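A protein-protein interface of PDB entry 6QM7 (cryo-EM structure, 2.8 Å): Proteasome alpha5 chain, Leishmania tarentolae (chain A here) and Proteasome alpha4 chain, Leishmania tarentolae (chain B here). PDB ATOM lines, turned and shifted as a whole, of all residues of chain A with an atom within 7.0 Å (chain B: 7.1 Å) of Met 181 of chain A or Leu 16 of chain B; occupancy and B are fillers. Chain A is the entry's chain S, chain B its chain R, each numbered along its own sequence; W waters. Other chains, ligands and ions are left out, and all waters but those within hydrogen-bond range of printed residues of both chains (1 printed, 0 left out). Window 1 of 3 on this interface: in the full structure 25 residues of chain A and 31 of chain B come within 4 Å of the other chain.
Met 181 of chain A touches just these residues of chain B: Phe 10 (3.8 Å) and Leu 16 (3.6 Å). Of chain A, only Met 181 (3.6 Å) and Arg 235 (3.4 Å) come within 4 Å of Leu 16 of chain B. Of the printed residues of chain A, Thr 119 of chain B touches Arg 235. Of the printed residues of chain A, Ser 150 of chain B touches Ala 183. Printed residues of chain B within 4 Å of Gln 123 of chain A: Val 9 (3.5 Å) and Phe 10 (2.7 Å). Of the printed residues of chain A, Thr 8 of chain B touches Arg 235. Of the printed residues of chain A, Gly 14 of chain B touches Ala 130 (3.2 Å). The nearest residue of chain B that does not touch Met 181 of chain A is Gly 14 of chain B (4.1 Å). The nearest printed residue of chain A that does not touch Met 152 of chain B is Val 182 of chain A (4.3 Å).
Gln 123 of chain A touches Val 9 of chain B. Phe 10 of chain B touches Ala 127 of chain A (CD1 to CA, 3.9 Å). Ala 130 of chain A touches Gly 14 of chain B (CB to O, 3.2 Å). CD1 of Leu 16 of chain B touches SD of Met 181 of chain A, 3.6 Å away. CD of Arg 235 of chain A touches O of Thr 8 of chain B, 3.5 Å away. Leu 16 of chain B touches Arg 235 of chain A (CD2 to CD, 3.4 Å). Pro 236 of chain A touches Phe 10 of chain B. Gln 120 of chain B touches Pro 236 of chain A (NE2 to O, 3.6 Å). Phe 237 of chain A touches Gln 120 of chain B (CE1 to OE1, 3.2 Å). Gly 238 of chain A touches Phe 10 of chain B (CA to CZ, 3.5 Å).
Of the 19 printed residues of chain B, 9 touch a printed residue of chain A. Hydrophobic or aromatic side chains of chain B within 4 Å of the printed part of chain A: Val 9, Phe 10 and Leu 16. Of the 20 printed residues of chain A, 9 touch a printed residue of chain B. Hydrophobic or aromatic side chains of chain A within 4 Å of the printed part of chain B: Ala 127, Ala 130, Met 181, Ala 183 and Phe 237. Among the printed residues, 18 pairs touch across the chains. Among the printed residues, no Asp or Glu carboxylate lies within 4 Å of a Lys or Arg side-chain nitrogen of the other chain.
The side-chain hydroxyl (OG) of Ser 150 of chain B is in hydrogen-bond range of the backbone NH (N) of Met 152 of chain B (3.3 Å). The backbone carbonyl oxygen (O) of Gly 238 of chain A sits at hydrogen-bond distance from the backbone NH (N) of Met 181 of chain A (3.2 Å). NH1 of Arg 235 of chain A is in salt-bridge range of OD2 of Asp 184 of chain A, 2.7 Å away. The backbone NH of Gly 238 of chain A is in hydrogen-bond range of the side-chain carboxylate of Asp 184 of chain A, at 3.2 Å.
The side-chain amide oxygen (OE1) of Gln 123 of chain A is in hydrogen-bond range of the backbone NH (N) of Phe 10 of chain B, 2.7 Å away. O of Thr 119 of chain B sits at hydrogen-bond distance from NE of Arg 235 of chain A (2.6 Å). The backbone carbonyl oxygen of Arg 235 of chain A is in hydrogen-bond range of the side-chain amide nitrogen of Gln 120 of chain B.
Water W1 bridges the side-chain carboxylate (OD1) of Asp 184 of chain A (2.6 Å) and the backbone carbonyl oxygen (O) of Ser 150 of chain B (3.0 Å).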
ATOM      1  N   GLN A 123      23.021  -1.042 -28.222  1.00  0.00           N
ATOM      2  CA  GLN A 123      23.010  -0.083 -27.087  1.00  0.00           C
ATOM      3  C   GLN A 123      24.022  -0.513 -26.026  1.00  0.00           C
ATOM      4  O   GLN A 123      24.668   0.389 -25.461  1.00  0.00           O
ATOM      5  CB  GLN A 123      21.626   0.057 -26.448  1.00  0.00           C
ATOM      6  CG  GLN A 123      20.672   0.931 -27.247  1.00  0.00           C
ATOM      7  CD  GLN A 123      21.217   2.313 -27.503  1.00  0.00           C
ATOM      8  OE1 GLN A 123      21.271   3.146 -26.601  1.00  0.00           O
ATOM      9  NE2 GLN A 123      21.619   2.563 -28.741  1.00  0.00           N
ATOM     10  N   ALA A 127      27.186   1.497 -24.958  1.00  0.00           N
ATOM     11  CA  ALA A 127      27.348   1.893 -23.540  1.00  0.00           C
ATOM     12  C   ALA A 127      28.760   1.526 -23.074  1.00  0.00           C
ATOM     13  O   ALA A 127      29.290   2.209 -22.191  1.00  0.00           O
ATOM     14  CB  ALA A 127      26.303   1.233 -22.671  1.00  0.00           C
ATOM     15  N   ALA A 130      31.188   4.114 -24.046  1.00  0.00           N
ATOM     16  CA  ALA A 130      31.023   5.255 -23.112  1.00  0.00           C
ATOM     17  C   ALA A 130      31.972   5.124 -21.922  1.00  0.00           C
ATOM     18  O   ALA A 130      32.383   6.165 -21.378  1.00  0.00           O
ATOM     19  CB  ALA A 130      29.593   5.348 -22.619  1.00  0.00           C
ATOM     20  N   ILE A 131      32.250   3.892 -21.499  1.00  0.00           N
ATOM     21  CA  ILE A 131      33.111   3.595 -20.320  1.00  0.00           C
ATOM     22  C   ILE A 131      34.565   3.873 -20.690  1.00  0.00           C
ATOM     23  O   ILE A 131      35.231   4.518 -19.873  1.00  0.00           O
ATOM     24  CB  ILE A 131      32.861   2.163 -19.817  1.00  0.00           C
ATOM     25  CG1 ILE A 131      31.488   2.079 -19.143  1.00  0.00           C
ATOM     26  CG2 ILE A 131      33.969   1.687 -18.892  1.00  0.00           C
ATOM     27  CD1 ILE A 131      30.798   0.751 -19.306  1.00  0.00           C
ATOM     28  N   GLY A 134      35.521   7.256 -19.983  1.00  0.00           N
ATOM     29  CA  GLY A 134      35.504   7.526 -18.533  1.00  0.00           C
ATOM     30  C   GLY A 134      36.876   7.435 -17.879  1.00  0.00           C
ATOM     31  O   GLY A 134      37.821   6.898 -18.497  1.00  0.00           O
ATOM     32  N   MET A 178      33.465   3.343  -9.766  1.00  0.00           N
ATOM     33  CA  MET A 178      32.771   3.487 -11.067  1.00  0.00           C
ATOM     34  C   MET A 178      33.742   3.999 -12.123  1.00  0.00           C
ATOM     35  O   MET A 178      34.751   4.648 -11.765  1.00  0.00           O
ATOM     36  CB  MET A 178      31.625   4.491 -10.975  1.00  0.00           C
ATOM     37  CG  MET A 178      32.077   5.914 -10.626  1.00  0.00           C
ATOM     38  SD  MET A 178      30.894   6.826  -9.580  1.00  0.00           S
ATOM     39  CE  MET A 178      30.642   5.674  -8.222  1.00  0.00           C
ATOM     40  N   SER A 179      33.421   3.710 -13.380  1.00  0.00           N
ATOM     41  CA  SER A 179      34.005   4.349 -14.581  1.00  0.00           C
ATOM     42  C   SER A 179      32.916   4.480 -15.630  1.00  0.00           C
ATOM     43  O   SER A 179      32.129   3.527 -15.773  1.00  0.00           O
ATOM     44  CB  SER A 179      35.165   3.584 -15.107  1.00  0.00           C
ATOM     45  OG  SER A 179      36.269   3.745 -14.236  1.00  0.00           O
ATOM     46  N   GLY A 180      32.912   5.610 -16.329  1.00  0.00           N
ATOM     47  CA  GLY A 180      31.836   5.996 -17.249  1.00  0.00           C
ATOM     48  C   GLY A 180      30.970   7.046 -16.608  1.00  0.00           C
ATOM     49  O   GLY A 180      31.507   7.882 -15.863  1.00  0.00           O
ATOM     50  N   MET A 181      29.675   7.006 -16.881  1.00  0.00           N
ATOM     51  CA  MET A 181      28.754   8.117 -16.545  1.00  0.00           C
ATOM     52  C   MET A 181      28.481   8.084 -15.041  1.00  0.00           C
ATOM     53  O   MET A 181      27.858   7.124 -14.548  1.00  0.00           O
ATOM     54  CB  MET A 181      27.451   8.006 -17.335  1.00  0.00           C
ATOM     55  CG  MET A 181      27.688   7.805 -18.803  1.00  0.00           C
ATOM     56  SD  MET A 181      26.216   8.205 -19.736  1.00  0.00           S
ATOM     57  CE  MET A 181      27.002   8.798 -21.238  1.00  0.00           C
ATOM     58  N   VAL A 182      28.966   9.104 -14.347  1.00  0.00           N
ATOM     59  CA  VAL A 182      29.035   9.132 -12.862  1.00  0.00           C
ATOM     60  C   VAL A 182      27.606   9.140 -12.320  1.00  0.00           C
ATOM     61  O   VAL A 182      27.313   8.323 -11.436  1.00  0.00           O
ATOM     62  CB  VAL A 182      29.854  10.344 -12.382  1.00  0.00           C
ATOM     63  CG1 VAL A 182      29.919  10.419 -10.859  1.00  0.00           C
ATOM     64  CG2 VAL A 182      31.254  10.326 -12.988  1.00  0.00           C
ATOM     65  N   ALA A 183      26.756  10.006 -12.868  1.00  0.00           N
ATOM     66  CA  ALA A 183      25.336  10.173 -12.480  1.00  0.00           C
ATOM     67  C   ALA A 183      24.620   8.822 -12.472  1.00  0.00           C
ATOM     68  O   ALA A 183      23.810   8.591 -11.567  1.00  0.00           O
ATOM     69  CB  ALA A 183      24.660  11.127 -13.425  1.00  0.00           C
ATOM     70  N   ASP A 184      24.894   7.991 -13.470  1.00  0.00           N
ATOM     71  CA  ASP A 184      24.308   6.638 -13.629  1.00  0.00           C
ATOM     72  C   ASP A 184      24.769   5.770 -12.453  1.00  0.00           C
ATOM     73  O   ASP A 184      23.902   5.207 -11.763  1.00  0.00           O
ATOM     74  CB  ASP A 184      24.699   6.041 -14.984  1.00  0.00           C
ATOM     75  CG  ASP A 184      24.159   6.802 -16.189  1.00  0.00           C
ATOM     76  OD1 ASP A 184      23.852   8.009 -16.038  1.00  0.00           O
ATOM     77  OD2 ASP A 184      24.078   6.193 -17.282  1.00  0.00           O
ATOM     78  N   ALA A 185      26.083   5.685 -12.223  1.00  0.00           N
ATOM     79  CA  ALA A 185      26.709   4.908 -11.124  1.00  0.00           C
ATOM     80  C   ALA A 185      26.000   5.199  -9.798  1.00  0.00           C
ATOM     81  O   ALA A 185      25.761   4.255  -9.030  1.00  0.00           O
ATOM     82  CB  ALA A 185      28.170   5.240 -11.010  1.00  0.00           C
ATOM     83  N   ARG A 186      25.676   6.463  -9.538  1.00  0.00           N
ATOM     84  CA  ARG A 186      24.995   6.901  -8.291  1.00  0.00           C
ATOM     85  C   ARG A 186      23.692   6.111  -8.145  1.00  0.00           C
ATOM     86  O   ARG A 186      23.328   5.826  -7.002  1.00  0.00           O
ATOM     87  CB  ARG A 186      24.713   8.408  -8.300  1.00  0.00           C
ATOM     88  CG  ARG A 186      25.947   9.289  -8.462  1.00  0.00           C
ATOM     89  CD  ARG A 186      26.459   9.895  -7.175  1.00  0.00           C
ATOM     90  NE  ARG A 186      27.858   9.552  -6.933  1.00  0.00           N
ATOM     91  CZ  ARG A 186      28.926  10.286  -7.264  1.00  0.00           C
ATOM     92  NH1 ARG A 186      28.798  11.454  -7.881  1.00  0.00           N
ATOM     93  NH2 ARG A 186      30.139   9.841  -6.965  1.00  0.00           N
ATOM     94  N   ARG A 235      17.585   3.300 -21.800  1.00  0.00           N
ATOM     95  CA  ARG A 235      18.935   2.884 -22.254  1.00  0.00           C
ATOM     96  C   ARG A 235      19.640   2.159 -21.121  1.00  0.00           C
ATOM     97  O   ARG A 235      19.240   2.304 -19.972  1.00  0.00           O
ATOM     98  CB  ARG A 235      19.786   4.111 -22.596  1.00  0.00           C
ATOM     99  CG  ARG A 235      19.846   5.123 -21.463  1.00  0.00           C
ATOM    100  CD  ARG A 235      20.762   6.271 -21.733  1.00  0.00           C
ATOM    101  NE  ARG A 235      20.740   7.174 -20.593  1.00  0.00           N
ATOM    102  CZ  ARG A 235      21.522   7.080 -19.526  1.00  0.00           C
ATOM    103  NH1 ARG A 235      22.427   6.115 -19.423  1.00  0.00           N
ATOM    104  NH2 ARG A 235      21.398   7.966 -18.555  1.00  0.00           N
ATOM    105  N   PRO A 236      20.735   1.415 -21.392  1.00  0.00           N
ATOM    106  CA  PRO A 236      21.556   0.877 -20.322  1.00  0.00           C
ATOM    107  C   PRO A 236      22.245   2.010 -19.554  1.00  0.00           C
ATOM    108  O   PRO A 236      22.232   3.137 -19.992  1.00  0.00           O
ATOM    109  CB  PRO A 236      22.559  -0.033 -21.041  1.00  0.00           C
ATOM    110  CG  PRO A 236      22.598   0.465 -22.452  1.00  0.00           C
ATOM    111  CD  PRO A 236      21.219   1.014 -22.720  1.00  0.00           C
ATOM    112  N   PHE A 237      22.792   1.679 -18.389  1.00  0.00           N
ATOM    113  CA  PHE A 237      23.735   2.555 -17.653  1.00  0.00           C
ATOM    114  C   PHE A 237      25.064   2.528 -18.405  1.00  0.00           C
ATOM    115  O   PHE A 237      25.535   1.439 -18.761  1.00  0.00           O
ATOM    116  CB  PHE A 237      23.905   2.096 -16.208  1.00  0.00           C
ATOM    117  CG  PHE A 237      22.651   2.142 -15.384  1.00  0.00           C
ATOM    118  CD1 PHE A 237      22.214   3.329 -14.820  1.00  0.00           C
ATOM    119  CD2 PHE A 237      21.915   1.001 -15.154  1.00  0.00           C
ATOM    120  CE1 PHE A 237      21.075   3.371 -14.030  1.00  0.00           C
ATOM    121  CE2 PHE A 237      20.783   1.041 -14.356  1.00  0.00           C
ATOM    122  CZ  PHE A 237      20.357   2.225 -13.803  1.00  0.00           C
ATOM    123  N   GLY A 238      25.629   3.709 -18.637  1.00  0.00           N
ATOM    124  CA  GLY A 238      26.923   3.885 -19.311  1.00  0.00           C
ATOM    125  C   GLY A 238      28.048   3.782 -18.315  1.00  0.00           C
ATOM    126  O   GLY A 238      29.113   4.356 -18.577  1.00  0.00           O
ATOM    127  N   VAL A 239      27.814   3.070 -17.219  1.00  0.00           N
ATOM    128  CA  VAL A 239      28.816   2.859 -16.147  1.00  0.00           C
ATOM    129  C   VAL A 239      29.161   1.372 -16.081  1.00  0.00           C
ATOM    130  O   VAL A 239      28.253   0.531 -16.258  1.00  0.00           O
ATOM    131  CB  VAL A 239      28.307   3.383 -14.794  1.00  0.00           C
ATOM    132  CG1 VAL A 239      27.146   2.569 -14.254  1.00  0.00           C
ATOM    133  CG2 VAL A 239      29.426   3.444 -13.761  1.00  0.00           C
ATOM    134  N   SER A 240      30.446   1.093 -15.856  1.00  0.00           N
ATOM    135  CA  SER A 240      30.973  -0.196 -15.348  1.00  0.00           C
ATOM    136  C   SER A 240      31.462   0.059 -13.936  1.00  0.00           C
ATOM    137  O   SER A 240      32.110   1.095 -13.727  1.00  0.00           O
ATOM    138  CB  SER A 240      32.085  -0.732 -16.200  1.00  0.00           C
ATOM    139  OG  SER A 240      32.436  -2.052 -15.817  1.00  0.00           O
ATOM    140  N   THR B   8      16.648   9.268 -25.042  1.00  0.00           N
ATOM    141  CA  THR B   8      18.080   9.372 -24.682  1.00  0.00           C
ATOM    142  C   THR B   8      18.692   7.990 -24.872  1.00  0.00           C
ATOM    143  O   THR B   8      18.324   7.083 -24.096  1.00  0.00           O
ATOM    144  CB  THR B   8      18.278   9.912 -23.263  1.00  0.00           C
ATOM    145  OG1 THR B   8      17.414  11.027 -23.016  1.00  0.00           O
ATOM    146  CG2 THR B   8      19.713  10.328 -23.033  1.00  0.00           C
ATOM    147  N   VAL B   9      19.536   7.834 -25.894  1.00  0.00           N
ATOM    148  CA  VAL B   9      20.114   6.525 -26.306  1.00  0.00           C
ATOM    149  C   VAL B   9      21.571   6.717 -26.691  1.00  0.00           C
ATOM    150  O   VAL B   9      21.953   7.821 -27.101  1.00  0.00           O
ATOM    151  CB  VAL B   9      19.316   5.892 -27.458  1.00  0.00           C
ATOM    152  CG1 VAL B   9      17.868   5.670 -27.057  1.00  0.00           C
ATOM    153  CG2 VAL B   9      19.405   6.702 -28.742  1.00  0.00           C
ATOM    154  N   PHE B  10      22.348   5.656 -26.574  1.00  0.00           N
ATOM    155  CA  PHE B  10      23.784   5.687 -26.904  1.00  0.00           C
ATOM    156  C   PHE B  10      23.924   5.663 -28.418  1.00  0.00           C
ATOM    157  O   PHE B  10      23.125   4.994 -29.101  1.00  0.00           O
ATOM    158  CB  PHE B  10      24.517   4.523 -26.247  1.00  0.00           C
ATOM    159  CG  PHE B  10      24.669   4.679 -24.763  1.00  0.00           C
ATOM    160  CD1 PHE B  10      25.757   5.341 -24.233  1.00  0.00           C
ATOM    161  CD2 PHE B  10      23.708   4.176 -23.902  1.00  0.00           C
ATOM    162  CE1 PHE B  10      25.873   5.494 -22.858  1.00  0.00           C
ATOM    163  CE2 PHE B  10      23.840   4.309 -22.533  1.00  0.00           C
ATOM    164  CZ  PHE B  10      24.915   4.980 -22.008  1.00  0.00           C
ATOM    165  N   SER B  11      24.921   6.395 -28.899  1.00  0.00           N
ATOM    166  CA  SER B  11      25.365   6.418 -30.309  1.00  0.00           C
ATOM    167  C   SER B  11      26.671   5.641 -30.410  1.00  0.00           C
ATOM    168  O   SER B  11      27.344   5.452 -29.402  1.00  0.00           O
ATOM    169  CB  SER B  11      25.517   7.835 -30.770  1.00  0.00           C
ATOM    170  OG  SER B  11      24.296   8.540 -30.586  1.00  0.00           O
ATOM    171  N   ASP B  13      29.774   6.132 -30.767  1.00  0.00           N
ATOM    172  CA  ASP B  13      31.006   6.625 -30.092  1.00  0.00           C
ATOM    173  C   ASP B  13      30.845   6.596 -28.561  1.00  0.00           C
ATOM    174  O   ASP B  13      31.802   6.999 -27.862  1.00  0.00           O
ATOM    175  CB  ASP B  13      31.390   8.017 -30.617  1.00  0.00           C
ATOM    176  CG  ASP B  13      32.402   8.014 -31.760  1.00  0.00           C
ATOM    177  OD1 ASP B  13      32.874   6.910 -32.137  1.00  0.00           O
ATOM    178  OD2 ASP B  13      32.724   9.122 -32.261  1.00  0.00           O
ATOM    179  N   GLY B  14      29.698   6.147 -28.046  1.00  0.00           N
ATOM    180  CA  GLY B  14      29.413   6.064 -26.600  1.00  0.00           C
ATOM    181  C   GLY B  14      28.729   7.308 -26.060  1.00  0.00           C
ATOM    182  O   GLY B  14      28.457   7.351 -24.845  1.00  0.00           O
ATOM    183  N   HIS B  15      28.424   8.272 -26.931  1.00  0.00           N
ATOM    184  CA  HIS B  15      27.791   9.564 -26.569  1.00  0.00           C
ATOM    185  C   HIS B  15      26.290   9.350 -26.386  1.00  0.00           C
ATOM    186  O   HIS B  15      25.708   8.576 -27.175  1.00  0.00           O
ATOM    187  CB  HIS B  15      28.099  10.616 -27.640  1.00  0.00           C
ATOM    188  CG  HIS B  15      29.558  10.917 -27.774  1.00  0.00           C
ATOM    189  ND1 HIS B  15      30.161  11.119 -29.004  1.00  0.00           N
ATOM    190  CD2 HIS B  15      30.531  11.036 -26.840  1.00  0.00           C
ATOM    191  CE1 HIS B  15      31.440  11.367 -28.818  1.00  0.00           C
ATOM    192  NE2 HIS B  15      31.694  11.317 -27.498  1.00  0.00           N
ATOM    193  N   LEU B  16      25.708   9.975 -25.359  1.00  0.00           N
ATOM    194  CA  LEU B  16      24.246  10.221 -25.258  1.00  0.00           C
ATOM    195  C   LEU B  16      23.951  11.556 -25.944  1.00  0.00           C
ATOM    196  O   LEU B  16      24.091  12.591 -25.282  1.00  0.00           O
ATOM    197  CB  LEU B  16      23.807  10.274 -23.792  1.00  0.00           C
ATOM    198  CG  LEU B  16      23.826   8.966 -23.003  1.00  0.00           C
ATOM    199  CD1 LEU B  16      23.315   9.198 -21.584  1.00  0.00           C
ATOM    200  CD2 LEU B  16      22.998   7.895 -23.674  1.00  0.00           C
ATOM    201  N   PHE B  17      23.582  11.538 -27.222  1.00  0.00           N
ATOM    202  CA  PHE B  17      23.413  12.771 -28.028  1.00  0.00           C
ATOM    203  C   PHE B  17      22.399  13.693 -27.355  1.00  0.00           C
ATOM    204  O   PHE B  17      22.627  14.909 -27.357  1.00  0.00           O
ATOM    205  CB  PHE B  17      23.019  12.467 -29.476  1.00  0.00           C
ATOM    206  CG  PHE B  17      24.166  12.164 -30.412  1.00  0.00           C
ATOM    207  CD1 PHE B  17      25.434  12.714 -30.226  1.00  0.00           C
ATOM    208  CD2 PHE B  17      23.956  11.359 -31.521  1.00  0.00           C
ATOM    209  CE1 PHE B  17      26.472  12.425 -31.097  1.00  0.00           C
ATOM    210  CE2 PHE B  17      24.997  11.079 -32.397  1.00  0.00           C
ATOM    211  CZ  PHE B  17      26.252  11.608 -32.183  1.00  0.00           C
ATOM    212  N   GLN B  18      21.342  13.142 -26.771  1.00  0.00           N
ATOM    213  CA  GLN B  18      20.221  13.952 -26.233  1.00  0.00           C
ATOM    214  C   GLN B  18      20.709  14.742 -25.023  1.00  0.00           C
ATOM    215  O   GLN B  18      20.181  15.836 -24.795  1.00  0.00           O
ATOM    216  CB  GLN B  18      19.009  13.063 -25.916  1.00  0.00           C
ATOM    217  CG  GLN B  18      17.673  13.584 -26.457  1.00  0.00           C
ATOM    218  CD  GLN B  18      17.744  14.113 -27.869  1.00  0.00           C
ATOM    219  OE1 GLN B  18      17.104  15.102 -28.196  1.00  0.00           O
ATOM    220  NE2 GLN B  18      18.544  13.478 -28.710  1.00  0.00           N
ATOM    221  N   VAL B  19      21.692  14.217 -24.297  1.00  0.00           N
ATOM    222  CA  VAL B  19      22.324  14.891 -23.127  1.00  0.00           C
ATOM    223  C   VAL B  19      23.351  15.909 -23.619  1.00  0.00           C
ATOM    224  O   VAL B  19      23.446  16.978 -23.007  1.00  0.00           O
ATOM    225  CB  VAL B  19      22.949  13.855 -22.179  1.00  0.00           C
ATOM    226  CG1 VAL B  19      23.890  14.484 -21.161  1.00  0.00           C
ATOM    227  CG2 VAL B  19      21.854  13.057 -21.491  1.00  0.00           C
ATOM    228  N   GLU B  20      24.104  15.577 -24.662  1.00  0.00           N
ATOM    229  CA  GLU B  20      25.087  16.498 -25.280  1.00  0.00           C
ATOM    230  C   GLU B  20      24.375  17.725 -25.847  1.00  0.00           C
ATOM    231  O   GLU B  20      24.997  18.794 -25.848  1.00  0.00           O
ATOM    232  CB  GLU B  20      25.898  15.779 -26.350  1.00  0.00           C
ATOM    233  CG  GLU B  20      26.902  14.793 -25.773  1.00  0.00           C
ATOM    234  CD  GLU B  20      27.967  14.341 -26.767  1.00  0.00           C
ATOM    235  OE1 GLU B  20      27.604  14.066 -27.944  1.00  0.00           O
ATOM    236  OE2 GLU B  20      29.161  14.281 -26.379  1.00  0.00           O
ATOM    237  N   TYR B  21      23.135  17.565 -26.310  1.00  0.00           N
ATOM    238  CA  TYR B  21      22.311  18.641 -26.919  1.00  0.00           C
ATOM    239  C   TYR B  21      21.637  19.453 -25.815  1.00  0.00           C
ATOM    240  O   TYR B  21      21.522  20.663 -25.955  1.00  0.00           O
ATOM    241  CB  TYR B  21      21.246  18.091 -27.873  1.00  0.00           C
ATOM    242  CG  TYR B  21      21.727  17.272 -29.048  1.00  0.00           C
ATOM    243  CD1 TYR B  21      23.029  17.358 -29.532  1.00  0.00           C
ATOM    244  CD2 TYR B  21      20.854  16.406 -29.699  1.00  0.00           C
ATOM    245  CE1 TYR B  21      23.444  16.597 -30.618  1.00  0.00           C
ATOM    246  CE2 TYR B  21      21.254  15.645 -30.788  1.00  0.00           C
ATOM    247  CZ  TYR B  21      22.555  15.739 -31.252  1.00  0.00           C
ATOM    248  OH  TYR B  21      22.955  14.984 -32.320  1.00  0.00           O
ATOM    249  N   ALA B  22      21.198  18.810 -24.739  1.00  0.00           N
ATOM    250  CA  ALA B  22      20.721  19.520 -23.535  1.00  0.00           C
ATOM    251  C   ALA B  22      21.844  20.407 -22.989  1.00  0.00           C
ATOM    252  O   ALA B  22      21.500  21.443 -22.431  1.00  0.00           O
ATOM    253  CB  ALA B  22      20.227  18.543 -22.499  1.00  0.00           C
ATOM    254  N   THR B 119      17.473  11.705 -18.278  1.00  0.00           N
ATOM    255  CA  THR B 119      18.386  11.144 -19.310  1.00  0.00           C
ATOM    256  C   THR B 119      18.178   9.640 -19.486  1.00  0.00           C
ATOM    257  O   THR B 119      18.928   9.072 -20.289  1.00  0.00           O
ATOM    258  CB  THR B 119      19.864  11.436 -19.019  1.00  0.00           C
ATOM    259  OG1 THR B 119      20.412  10.480 -18.109  1.00  0.00           O
ATOM    260  CG2 THR B 119      20.081  12.832 -18.479  1.00  0.00           C
ATOM    261  N   GLN B 120      17.268   9.010 -18.737  1.00  0.00           N
ATOM    262  CA  GLN B 120      17.053   7.536 -18.780  1.00  0.00           C
ATOM    263  C   GLN B 120      15.563   7.180 -18.771  1.00  0.00           C
ATOM    264  O   GLN B 120      15.247   6.007 -18.992  1.00  0.00           O
ATOM    265  CB  GLN B 120      17.775   6.858 -17.613  1.00  0.00           C
ATOM    266  CG  GLN B 120      18.441   5.534 -17.986  1.00  0.00           C
ATOM    267  CD  GLN B 120      19.304   4.973 -16.878  1.00  0.00           C
ATOM    268  OE1 GLN B 120      19.300   5.466 -15.750  1.00  0.00           O
ATOM    269  NE2 GLN B 120      20.055   3.931 -17.193  1.00  0.00           N
ATOM    270  N   PRO B 126      16.031  14.960 -21.785  1.00  0.00           N
ATOM    271  CA  PRO B 126      16.618  15.540 -20.588  1.00  0.00           C
ATOM    272  C   PRO B 126      16.093  16.957 -20.310  1.00  0.00           C
ATOM    273  O   PRO B 126      15.565  17.594 -21.204  1.00  0.00           O
ATOM    274  CB  PRO B 126      18.105  15.577 -20.937  1.00  0.00           C
ATOM    275  CG  PRO B 126      18.265  14.447 -21.901  1.00  0.00           C
ATOM    276  CD  PRO B 126      17.043  14.577 -22.776  1.00  0.00           C
ATOM    277  N   SER B 150      23.381  15.967 -17.521  1.00  0.00           N
ATOM    278  CA  SER B 150      23.692  14.524 -17.331  1.00  0.00           C
ATOM    279  C   SER B 150      23.192  14.042 -15.963  1.00  0.00           C
ATOM    280  O   SER B 150      22.955  12.832 -15.808  1.00  0.00           O
ATOM    281  CB  SER B 150      25.166  14.250 -17.491  1.00  0.00           C
ATOM    282  OG  SER B 150      25.906  14.822 -16.427  1.00  0.00           O
ATOM    283  N   MET B 152      24.984  14.852 -13.264  1.00  0.00           N
ATOM    284  CA  MET B 152      26.254  14.705 -12.535  1.00  0.00           C
ATOM    285  C   MET B 152      26.465  16.040 -11.828  1.00  0.00           C
ATOM    286  O   MET B 152      26.267  17.074 -12.462  1.00  0.00           O
ATOM    287  CB  MET B 152      27.382  14.275 -13.488  1.00  0.00           C
ATOM    288  CG  MET B 152      28.561  15.197 -13.636  1.00  0.00           C
ATOM    289  SD  MET B 152      29.925  14.621 -12.609  1.00  0.00           S
ATOM    290  CE  MET B 152      30.998  16.060 -12.691  1.00  0.00           C
HETATM  291  O   HOH W   1      23.785  10.328 -17.184  1.00  0.00           O
